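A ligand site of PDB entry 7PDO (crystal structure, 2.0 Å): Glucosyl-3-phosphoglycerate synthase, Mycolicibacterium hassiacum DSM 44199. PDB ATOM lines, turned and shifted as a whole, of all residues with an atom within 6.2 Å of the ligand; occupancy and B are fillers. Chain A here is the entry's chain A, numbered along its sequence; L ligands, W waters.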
ATOM      1  N   PRO A  47      20.018  22.902   1.804  1.00  0.00           N
ATOM      2  CA  PRO A  47      20.114  21.594   1.150  1.00  0.00           C
ATOM      3  C   PRO A  47      19.826  20.514   2.175  1.00  0.00           C
ATOM      4  O   PRO A  47      20.239  20.617   3.334  1.00  0.00           O
ATOM      5  CB  PRO A  47      21.578  21.546   0.686  1.00  0.00           C
ATOM      6  CG  PRO A  47      22.304  22.309   1.759  1.00  0.00           C
ATOM      7  CD  PRO A  47      21.343  23.433   2.179  1.00  0.00           C
ATOM      8  N   ALA A  48      19.125  19.462   1.752  1.00  0.00           N
ATOM      9  CA  ALA A  48      18.744  18.410   2.698  1.00  0.00           C
ATOM     10  C   ALA A  48      18.682  17.061   2.005  1.00  0.00           C
ATOM     11  O   ALA A  48      17.871  16.851   1.089  1.00  0.00           O
ATOM     12  CB  ALA A  48      17.404  18.722   3.363  1.00  0.00           C
ATOM     13  N   LEU A  49      19.518  16.134   2.466  1.00  0.00           N
ATOM     14  CA  LEU A  49      19.456  14.731   2.102  1.00  0.00           C
ATOM     15  C   LEU A  49      19.249  13.916   3.382  1.00  0.00           C
ATOM     16  O   LEU A  49      20.185  13.768   4.177  1.00  0.00           O
ATOM     17  CB  LEU A  49      20.723  14.291   1.366  1.00  0.00           C
ATOM     18  CG  LEU A  49      20.776  12.806   1.016  1.00  0.00           C
ATOM     19  CD1 LEU A  49      19.581  12.433   0.161  1.00  0.00           C
ATOM     20  CD2 LEU A  49      22.069  12.483   0.296  1.00  0.00           C
ATOM     21  N   ASN A  50      18.040  13.413   3.573  1.00  0.00           N
ATOM     22  CA  ASN A  50      17.698  12.546   4.707  1.00  0.00           C
ATOM     23  C   ASN A  50      18.093  13.171   6.047  1.00  0.00           C
ATOM     24  O   ASN A  50      18.910  12.640   6.792  1.00  0.00           O
ATOM     25  CB  ASN A  50      18.326  11.164   4.535  1.00  0.00           C
ATOM     26  CG  ASN A  50      17.738  10.413   3.372  1.00  0.00           C
ATOM     27  OD1 ASN A  50      16.528  10.445   3.141  1.00  0.00           O
ATOM     28  ND2 ASN A  50      18.600   9.739   2.610  1.00  0.00           N
ATOM     29  N   GLU A  51      17.501  14.319   6.343  1.00  0.00           N
ATOM     30  CA  GLU A  51      17.785  15.040   7.574  1.00  0.00           C
ATOM     31  C   GLU A  51      16.531  15.176   8.435  1.00  0.00           C
ATOM     32  O   GLU A  51      16.270  16.227   9.020  1.00  0.00           O
ATOM     33  CB  GLU A  51      18.376  16.417   7.274  1.00  0.00           C
ATOM     34  CG  GLU A  51      19.608  16.385   6.329  1.00  0.00           C
ATOM     35  CD  GLU A  51      20.860  15.787   6.976  1.00  0.00           C
ATOM     36  OE1 GLU A  51      20.803  15.442   8.179  1.00  0.00           O
ATOM     37  OE2 GLU A  51      21.902  15.683   6.305  1.00  0.00           O
ATOM     38  N   LEU A  76      15.878  22.513  -0.224  1.00  0.00           N
ATOM     39  CA  LEU A  76      16.103  21.841  -1.488  1.00  0.00           C
ATOM     40  C   LEU A  76      16.357  20.361  -1.193  1.00  0.00           C
ATOM     41  O   LEU A  76      17.457  19.969  -0.788  1.00  0.00           O
ATOM     42  CB  LEU A  76      17.247  22.462  -2.266  1.00  0.00           C
ATOM     43  CG  LEU A  76      16.634  22.305  -3.662  1.00  0.00           C
ATOM     44  CD1 LEU A  76      16.561  23.586  -4.394  1.00  0.00           C
ATOM     45  CD2 LEU A  76      17.296  21.177  -4.417  1.00  0.00           C
ATOM     46  N   ASP A  77      15.311  19.554  -1.391  1.00  0.00           N
ATOM     47  CA  ASP A  77      15.344  18.145  -1.086  1.00  0.00           C
ATOM     48  C   ASP A  77      16.204  17.423  -2.111  1.00  0.00           C
ATOM     49  O   ASP A  77      15.968  17.539  -3.320  1.00  0.00           O
ATOM     50  CB  ASP A  77      13.921  17.589  -1.092  1.00  0.00           C
ATOM     51  CG  ASP A  77      13.826  16.139  -0.646  1.00  0.00           C
ATOM     52  OD1 ASP A  77      14.871  15.517  -0.362  1.00  0.00           O
ATOM     53  OD2 ASP A  77      12.685  15.627  -0.578  1.00  0.00           O
ATOM     54  N   SER A  78      17.198  16.684  -1.628  1.00  0.00           N
ATOM     55  CA  SER A  78      18.219  16.088  -2.474  1.00  0.00           C
ATOM     56  C   SER A  78      17.954  14.617  -2.757  1.00  0.00           C
ATOM     57  O   SER A  78      18.898  13.844  -2.941  1.00  0.00           O
ATOM     58  CB  SER A  78      19.595  16.263  -1.809  1.00  0.00           C
ATOM     59  OG  SER A  78      20.607  15.718  -2.630  1.00  0.00           O
ATOM     60  N   ARG A  98      15.117  18.411  -6.444  1.00  0.00           N
ATOM     61  CA  ARG A  98      16.093  18.761  -7.487  1.00  0.00           C
ATOM     62  C   ARG A  98      15.418  18.789  -8.854  1.00  0.00           C
ATOM     63  O   ARG A  98      15.704  19.672  -9.668  1.00  0.00           O
ATOM     64  CB  ARG A  98      17.261  17.783  -7.481  1.00  0.00           C
ATOM     65  CG  ARG A  98      18.069  17.851  -6.167  1.00  0.00           C
ATOM     66  CD  ARG A  98      19.043  16.686  -6.026  1.00  0.00           C
ATOM     67  NE  ARG A  98      18.349  15.398  -6.080  1.00  0.00           N
ATOM     68  CZ  ARG A  98      18.955  14.220  -6.146  1.00  0.00           C
ATOM     69  NH1 ARG A  98      20.274  14.117  -6.133  1.00  0.00           N
ATOM     70  NH2 ARG A  98      18.217  13.118  -6.243  1.00  0.00           N
ATOM     71  N   PRO A 109      24.437  13.274  -8.147  1.00  0.00           N
ATOM     72  CA  PRO A 109      24.555  13.207  -6.696  1.00  0.00           C
ATOM     73  C   PRO A 109      25.434  14.326  -6.162  1.00  0.00           C
ATOM     74  O   PRO A 109      26.285  14.884  -6.857  1.00  0.00           O
ATOM     75  CB  PRO A 109      25.208  11.833  -6.442  1.00  0.00           C
ATOM     76  CG  PRO A 109      25.121  11.101  -7.739  1.00  0.00           C
ATOM     77  CD  PRO A 109      25.075  12.125  -8.817  1.00  0.00           C
ATOM     78  N   GLY A 110      25.215  14.665  -4.898  1.00  0.00           N
ATOM     79  CA  GLY A 110      26.165  15.500  -4.210  1.00  0.00           C
ATOM     80  C   GLY A 110      25.559  16.844  -3.831  1.00  0.00           C
ATOM     81  O   GLY A 110      24.586  17.319  -4.418  1.00  0.00           O
ATOM     82  N   LYS A 111      26.194  17.473  -2.838  1.00  0.00           N
ATOM     83  CA  LYS A 111      25.689  18.729  -2.306  1.00  0.00           C
ATOM     84  C   LYS A 111      25.825  19.866  -3.324  1.00  0.00           C
ATOM     85  O   LYS A 111      24.935  20.710  -3.431  1.00  0.00           O
ATOM     86  CB  LYS A 111      26.448  19.067  -1.019  1.00  0.00           C
ATOM     87  CG  LYS A 111      25.916  20.289  -0.308  1.00  0.00           C
ATOM     88  CD  LYS A 111      26.863  20.704   0.817  1.00  0.00           C
ATOM     89  CE  LYS A 111      26.199  21.707   1.741  1.00  0.00           C
ATOM     90  NZ  LYS A 111      27.186  22.570   2.473  1.00  0.00           N
ATOM     91  N   VAL A 114      22.896  20.338  -5.522  1.00  0.00           N
ATOM     92  CA  VAL A 114      21.711  20.878  -4.845  1.00  0.00           C
ATOM     93  C   VAL A 114      21.763  22.399  -4.824  1.00  0.00           C
ATOM     94  O   VAL A 114      20.790  23.081  -5.162  1.00  0.00           O
ATOM     95  CB  VAL A 114      21.612  20.293  -3.426  1.00  0.00           C
ATOM     96  CG1 VAL A 114      20.468  20.941  -2.675  1.00  0.00           C
ATOM     97  CG2 VAL A 114      21.428  18.789  -3.500  1.00  0.00           C
ATOM     98  N   ILE A 130      22.336  27.401   4.358  1.00  0.00           N
ATOM     99  CA  ILE A 130      22.402  26.918   5.739  1.00  0.00           C
ATOM    100  C   ILE A 130      22.256  25.399   5.707  1.00  0.00           C
ATOM    101  O   ILE A 130      21.288  24.890   5.135  1.00  0.00           O
ATOM    102  CB  ILE A 130      21.288  27.504   6.636  1.00  0.00           C
ATOM    103  CG1 ILE A 130      21.307  29.031   6.624  1.00  0.00           C
ATOM    104  CG2 ILE A 130      21.435  26.965   8.083  1.00  0.00           C
ATOM    105  CD1 ILE A 130      22.450  29.640   7.417  1.00  0.00           C
ATOM    106  N   ASP A 131      23.192  24.679   6.330  1.00  0.00           N
ATOM    107  CA  ASP A 131      23.094  23.231   6.373  1.00  0.00           C
ATOM    108  C   ASP A 131      21.886  22.808   7.184  1.00  0.00           C
ATOM    109  O   ASP A 131      21.519  23.458   8.176  1.00  0.00           O
ATOM    110  CB  ASP A 131      24.362  22.618   6.977  1.00  0.00           C
ATOM    111  CG  ASP A 131      25.518  22.560   5.994  1.00  0.00           C
ATOM    112  OD1 ASP A 131      25.273  22.636   4.768  1.00  0.00           O
ATOM    113  OD2 ASP A 131      26.681  22.432   6.455  1.00  0.00           O
ATOM    114  N   SER A 132      21.244  21.732   6.763  1.00  0.00           N
ATOM    115  CA  SER A 132      20.040  21.262   7.437  1.00  0.00           C
ATOM    116  C   SER A 132      20.328  20.203   8.491  1.00  0.00           C
ATOM    117  O   SER A 132      19.390  19.726   9.159  1.00  0.00           O
ATOM    118  CB  SER A 132      19.044  20.711   6.405  1.00  0.00           C
ATOM    119  OG  SER A 132      19.630  19.622   5.713  1.00  0.00           O
ATOM    120  N   ASP A 133      21.593  19.799   8.650  1.00  0.00           N
ATOM    121  CA  ASP A 133      21.935  18.811   9.658  1.00  0.00           C
ATOM    122  C   ASP A 133      22.388  19.438  10.965  1.00  0.00           C
ATOM    123  O   ASP A 133      22.814  18.714  11.870  1.00  0.00           O
ATOM    124  CB  ASP A 133      23.003  17.857   9.133  1.00  0.00           C
ATOM    125  CG  ASP A 133      24.296  18.562   8.796  1.00  0.00           C
ATOM    126  OD1 ASP A 133      24.320  19.810   8.725  1.00  0.00           O
ATOM    127  OD2 ASP A 133      25.301  17.854   8.611  1.00  0.00           O
ATOM    128  N   LEU A 134      22.319  20.760  11.086  1.00  0.00           N
ATOM    129  CA  LEU A 134      22.773  21.428  12.306  1.00  0.00           C
ATOM    130  C   LEU A 134      21.898  21.034  13.483  1.00  0.00           C
ATOM    131  O   LEU A 134      20.674  21.164  13.414  1.00  0.00           O
ATOM    132  CB  LEU A 134      22.734  22.941  12.123  1.00  0.00           C
ATOM    133  CG  LEU A 134      23.517  23.469  10.935  1.00  0.00           C
ATOM    134  CD1 LEU A 134      23.508  24.997  10.936  1.00  0.00           C
ATOM    135  CD2 LEU A 134      24.932  22.895  10.946  1.00  0.00           C
ATOM    136  N   TYR A 223      31.200  17.478  -2.243  1.00  0.00           N
ATOM    137  CA  TYR A 223      31.715  18.278  -1.146  1.00  0.00           C
ATOM    138  C   TYR A 223      32.736  19.318  -1.581  1.00  0.00           C
ATOM    139  O   TYR A 223      33.236  20.058  -0.734  1.00  0.00           O
ATOM    140  CB  TYR A 223      32.317  17.385  -0.065  1.00  0.00           C
ATOM    141  CG  TYR A 223      31.249  16.578   0.644  1.00  0.00           C
ATOM    142  CD1 TYR A 223      30.180  17.212   1.272  1.00  0.00           C
ATOM    143  CD2 TYR A 223      31.288  15.186   0.645  1.00  0.00           C
ATOM    144  CE1 TYR A 223      29.187  16.480   1.901  1.00  0.00           C
ATOM    145  CE2 TYR A 223      30.315  14.448   1.279  1.00  0.00           C
ATOM    146  CZ  TYR A 223      29.261  15.099   1.907  1.00  0.00           C
ATOM    147  OH  TYR A 223      28.284  14.353   2.514  1.00  0.00           O
ATOM    148  N   ARG A 253      31.239  18.418  15.348  1.00  0.00           N
ATOM    149  CA  ARG A 253      30.753  17.078  15.095  1.00  0.00           C
ATOM    150  C   ARG A 253      31.856  16.044  15.339  1.00  0.00           C
ATOM    151  O   ARG A 253      33.015  16.375  15.630  1.00  0.00           O
ATOM    152  CB  ARG A 253      30.237  16.965  13.661  1.00  0.00           C
ATOM    153  CG  ARG A 253      29.127  17.956  13.311  1.00  0.00           C
ATOM    154  CD  ARG A 253      28.897  18.060  11.798  1.00  0.00           C
ATOM    155  NE  ARG A 253      29.798  19.016  11.155  1.00  0.00           N
ATOM    156  CZ  ARG A 253      29.727  19.382   9.890  1.00  0.00           C
ATOM    157  NH1 ARG A 253      28.812  18.872   9.069  1.00  0.00           N
ATOM    158  NH2 ARG A 253      30.603  20.276   9.419  1.00  0.00           N
ATOM    159  N   ARG A 255      32.431  13.075  13.000  1.00  0.00           N
ATOM    160  CA  ARG A 255      32.248  12.231  11.820  1.00  0.00           C
ATOM    161  C   ARG A 255      33.391  11.220  11.706  1.00  0.00           C
ATOM    162  O   ARG A 255      34.502  11.463  12.173  1.00  0.00           O
ATOM    163  CB  ARG A 255      32.163  13.084  10.558  1.00  0.00           C
ATOM    164  CG  ARG A 255      30.937  13.982  10.525  1.00  0.00           C
ATOM    165  CD  ARG A 255      30.908  14.899   9.316  1.00  0.00           C
ATOM    166  NE  ARG A 255      31.897  15.964   9.425  1.00  0.00           N
ATOM    167  CZ  ARG A 255      32.040  16.955   8.551  1.00  0.00           C
ATOM    168  NH1 ARG A 255      31.275  17.036   7.471  1.00  0.00           N
ATOM    169  NH2 ARG A 255      32.971  17.874   8.756  1.00  0.00           N
HETATM  170  N1  LIG L   1      23.553  17.267   1.490  1.00  0.00           N
HETATM  171  C1  LIG L   1      22.638  17.291   0.448  1.00  0.00           C
HETATM  172  N2  LIG L   1      22.924  16.447  -0.594  1.00  0.00           N
HETATM  173  C2  LIG L   1      23.985  15.585  -0.688  1.00  0.00           C
HETATM  174  C3  LIG L   1      24.890  15.613   0.424  1.00  0.00           C
HETATM  175  C4  LIG L   1      24.653  16.436   1.455  1.00  0.00           C
HETATM  176  O1  LIG L   1      21.654  18.010   0.454  1.00  0.00           O
HETATM  177  O2  LIG L   1      24.108  14.861  -1.693  1.00  0.00           O
HETATM  178  C5  LIG L   1      23.311  18.150   2.639  1.00  0.00           C
HETATM  179  C6  LIG L   1      23.182  17.409   3.973  1.00  0.00           C
HETATM  180  O3  LIG L   1      21.811  17.055   4.178  1.00  0.00           O
HETATM  181  C7  LIG L   1      23.629  18.484   4.971  1.00  0.00           C
HETATM  182  C8  LIG L   1      24.714  19.233   4.192  1.00  0.00           C
HETATM  183  O4  LIG L   1      24.421  19.025   2.784  1.00  0.00           O
HETATM  184  O5  LIG L   1      22.566  19.372   5.274  1.00  0.00           O
HETATM  185  C9  LIG L   1      26.141  18.820   4.485  1.00  0.00           C
HETATM  186  O6  LIG L   1      26.258  17.398   4.269  1.00  0.00           O
HETATM  187  P1  LIG L   1      26.900  16.445   5.366  1.00  0.00           P
HETATM  188  O7  LIG L   1      27.931  17.200   6.201  1.00  0.00           O
HETATM  189  O8  LIG L   1      27.357  15.231   4.652  1.00  0.00           O
HETATM  190  O9  LIG L   1      25.667  16.082   6.367  1.00  0.00           O
HETATM  191  P2  LIG L   1      25.333  14.713   7.099  1.00  0.00           P
HETATM  192  O10 LIG L   1      25.246  15.120   8.602  1.00  0.00           O
HETATM  193  O11 LIG L   1      26.603  13.877   6.867  1.00  0.00           O
HETATM  194  O12 LIG L   1      24.046  14.067   6.576  1.00  0.00           O
HETATM  195  O   HOH W   1      22.868  13.469  -3.492  1.00  0.00           O
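O3 of the ligand sits at hydrogen-bond distance from N of Leu 49, 3.0 Å away.
O5 of the ligand is in hydrogen-bond range of O of Pro 47 (3.3 Å).
An oxygen (O7) of the ligand lies within salt-bridge range of the guanidinium group (NH1) of Arg 255 (3.6 Å).
OH of Tyr 223 lies within hydrogen-bond range of O8 of the ligand (2.5 Å).
A nitrogen (N2) of the ligand lies within hydrogen-bond range of the side-chain hydroxyl (OG) of Ser 78 (3.2 Å).
An oxygen (O7) of the ligand is in salt-bridge range of the guanidinium group of Arg 253, at 3.4 Å.
O1 of the ligand lies within hydrogen-bond range of N of Ala 48 (3.2 Å).
OE2 of Glu 51 lies within hydrogen-bond range of O3 of the ligand.
OG of Ser 132 sits at hydrogen-bond distance from O5 of the ligand, at 3.0 Å.
N of Ser 132 lies within hydrogen-bond range of O5 of the ligand, at 3.1 Å.
An oxygen (O2) of the ligand sits close to the backbone NH (N) of Gly 110 (3.4 Å).
An oxygen (O10) of the ligand lies close to the side-chain carboxylate (OD2) of Asp 133, at 2.7 Å.
The backbone carbonyl oxygen (O) of Ser 78 sits close to the guanidinium group (NH2) of Arg 98 (3.4 Å).
O of Pro 47 lies within hydrogen-bond range of OG of Ser 132, 2.6 Å away.
NZ of Lys 111 lies within salt-bridge range of OD1 of Asp 131.
OD2 of Asp 133 lies within salt-bridge range of NH1 of Arg 253.
The backbone NH (N) of Ser 78 is in hydrogen-bond range of the backbone carbonyl oxygen (O) of Ala 48 (2.8 Å).
The backbone carbonyl oxygen of Leu 76 is in hydrogen-bond range of the backbone NH of Ala 48, 3.1 Å away.
Residues that only touch the ligand: Lys 111 and Asp 131.
Of the 21 residues printed, 13 come within 4 Å of the ligand.
Along chain A the residues within 4 Å of the ligand span positions 47 to 255.
Water W1 lies within hydrogen-bond range of O2 of the ligand (2.6 Å), N of Gly 110 (3.0 Å) and OG of Ser 78 (3.3 Å).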
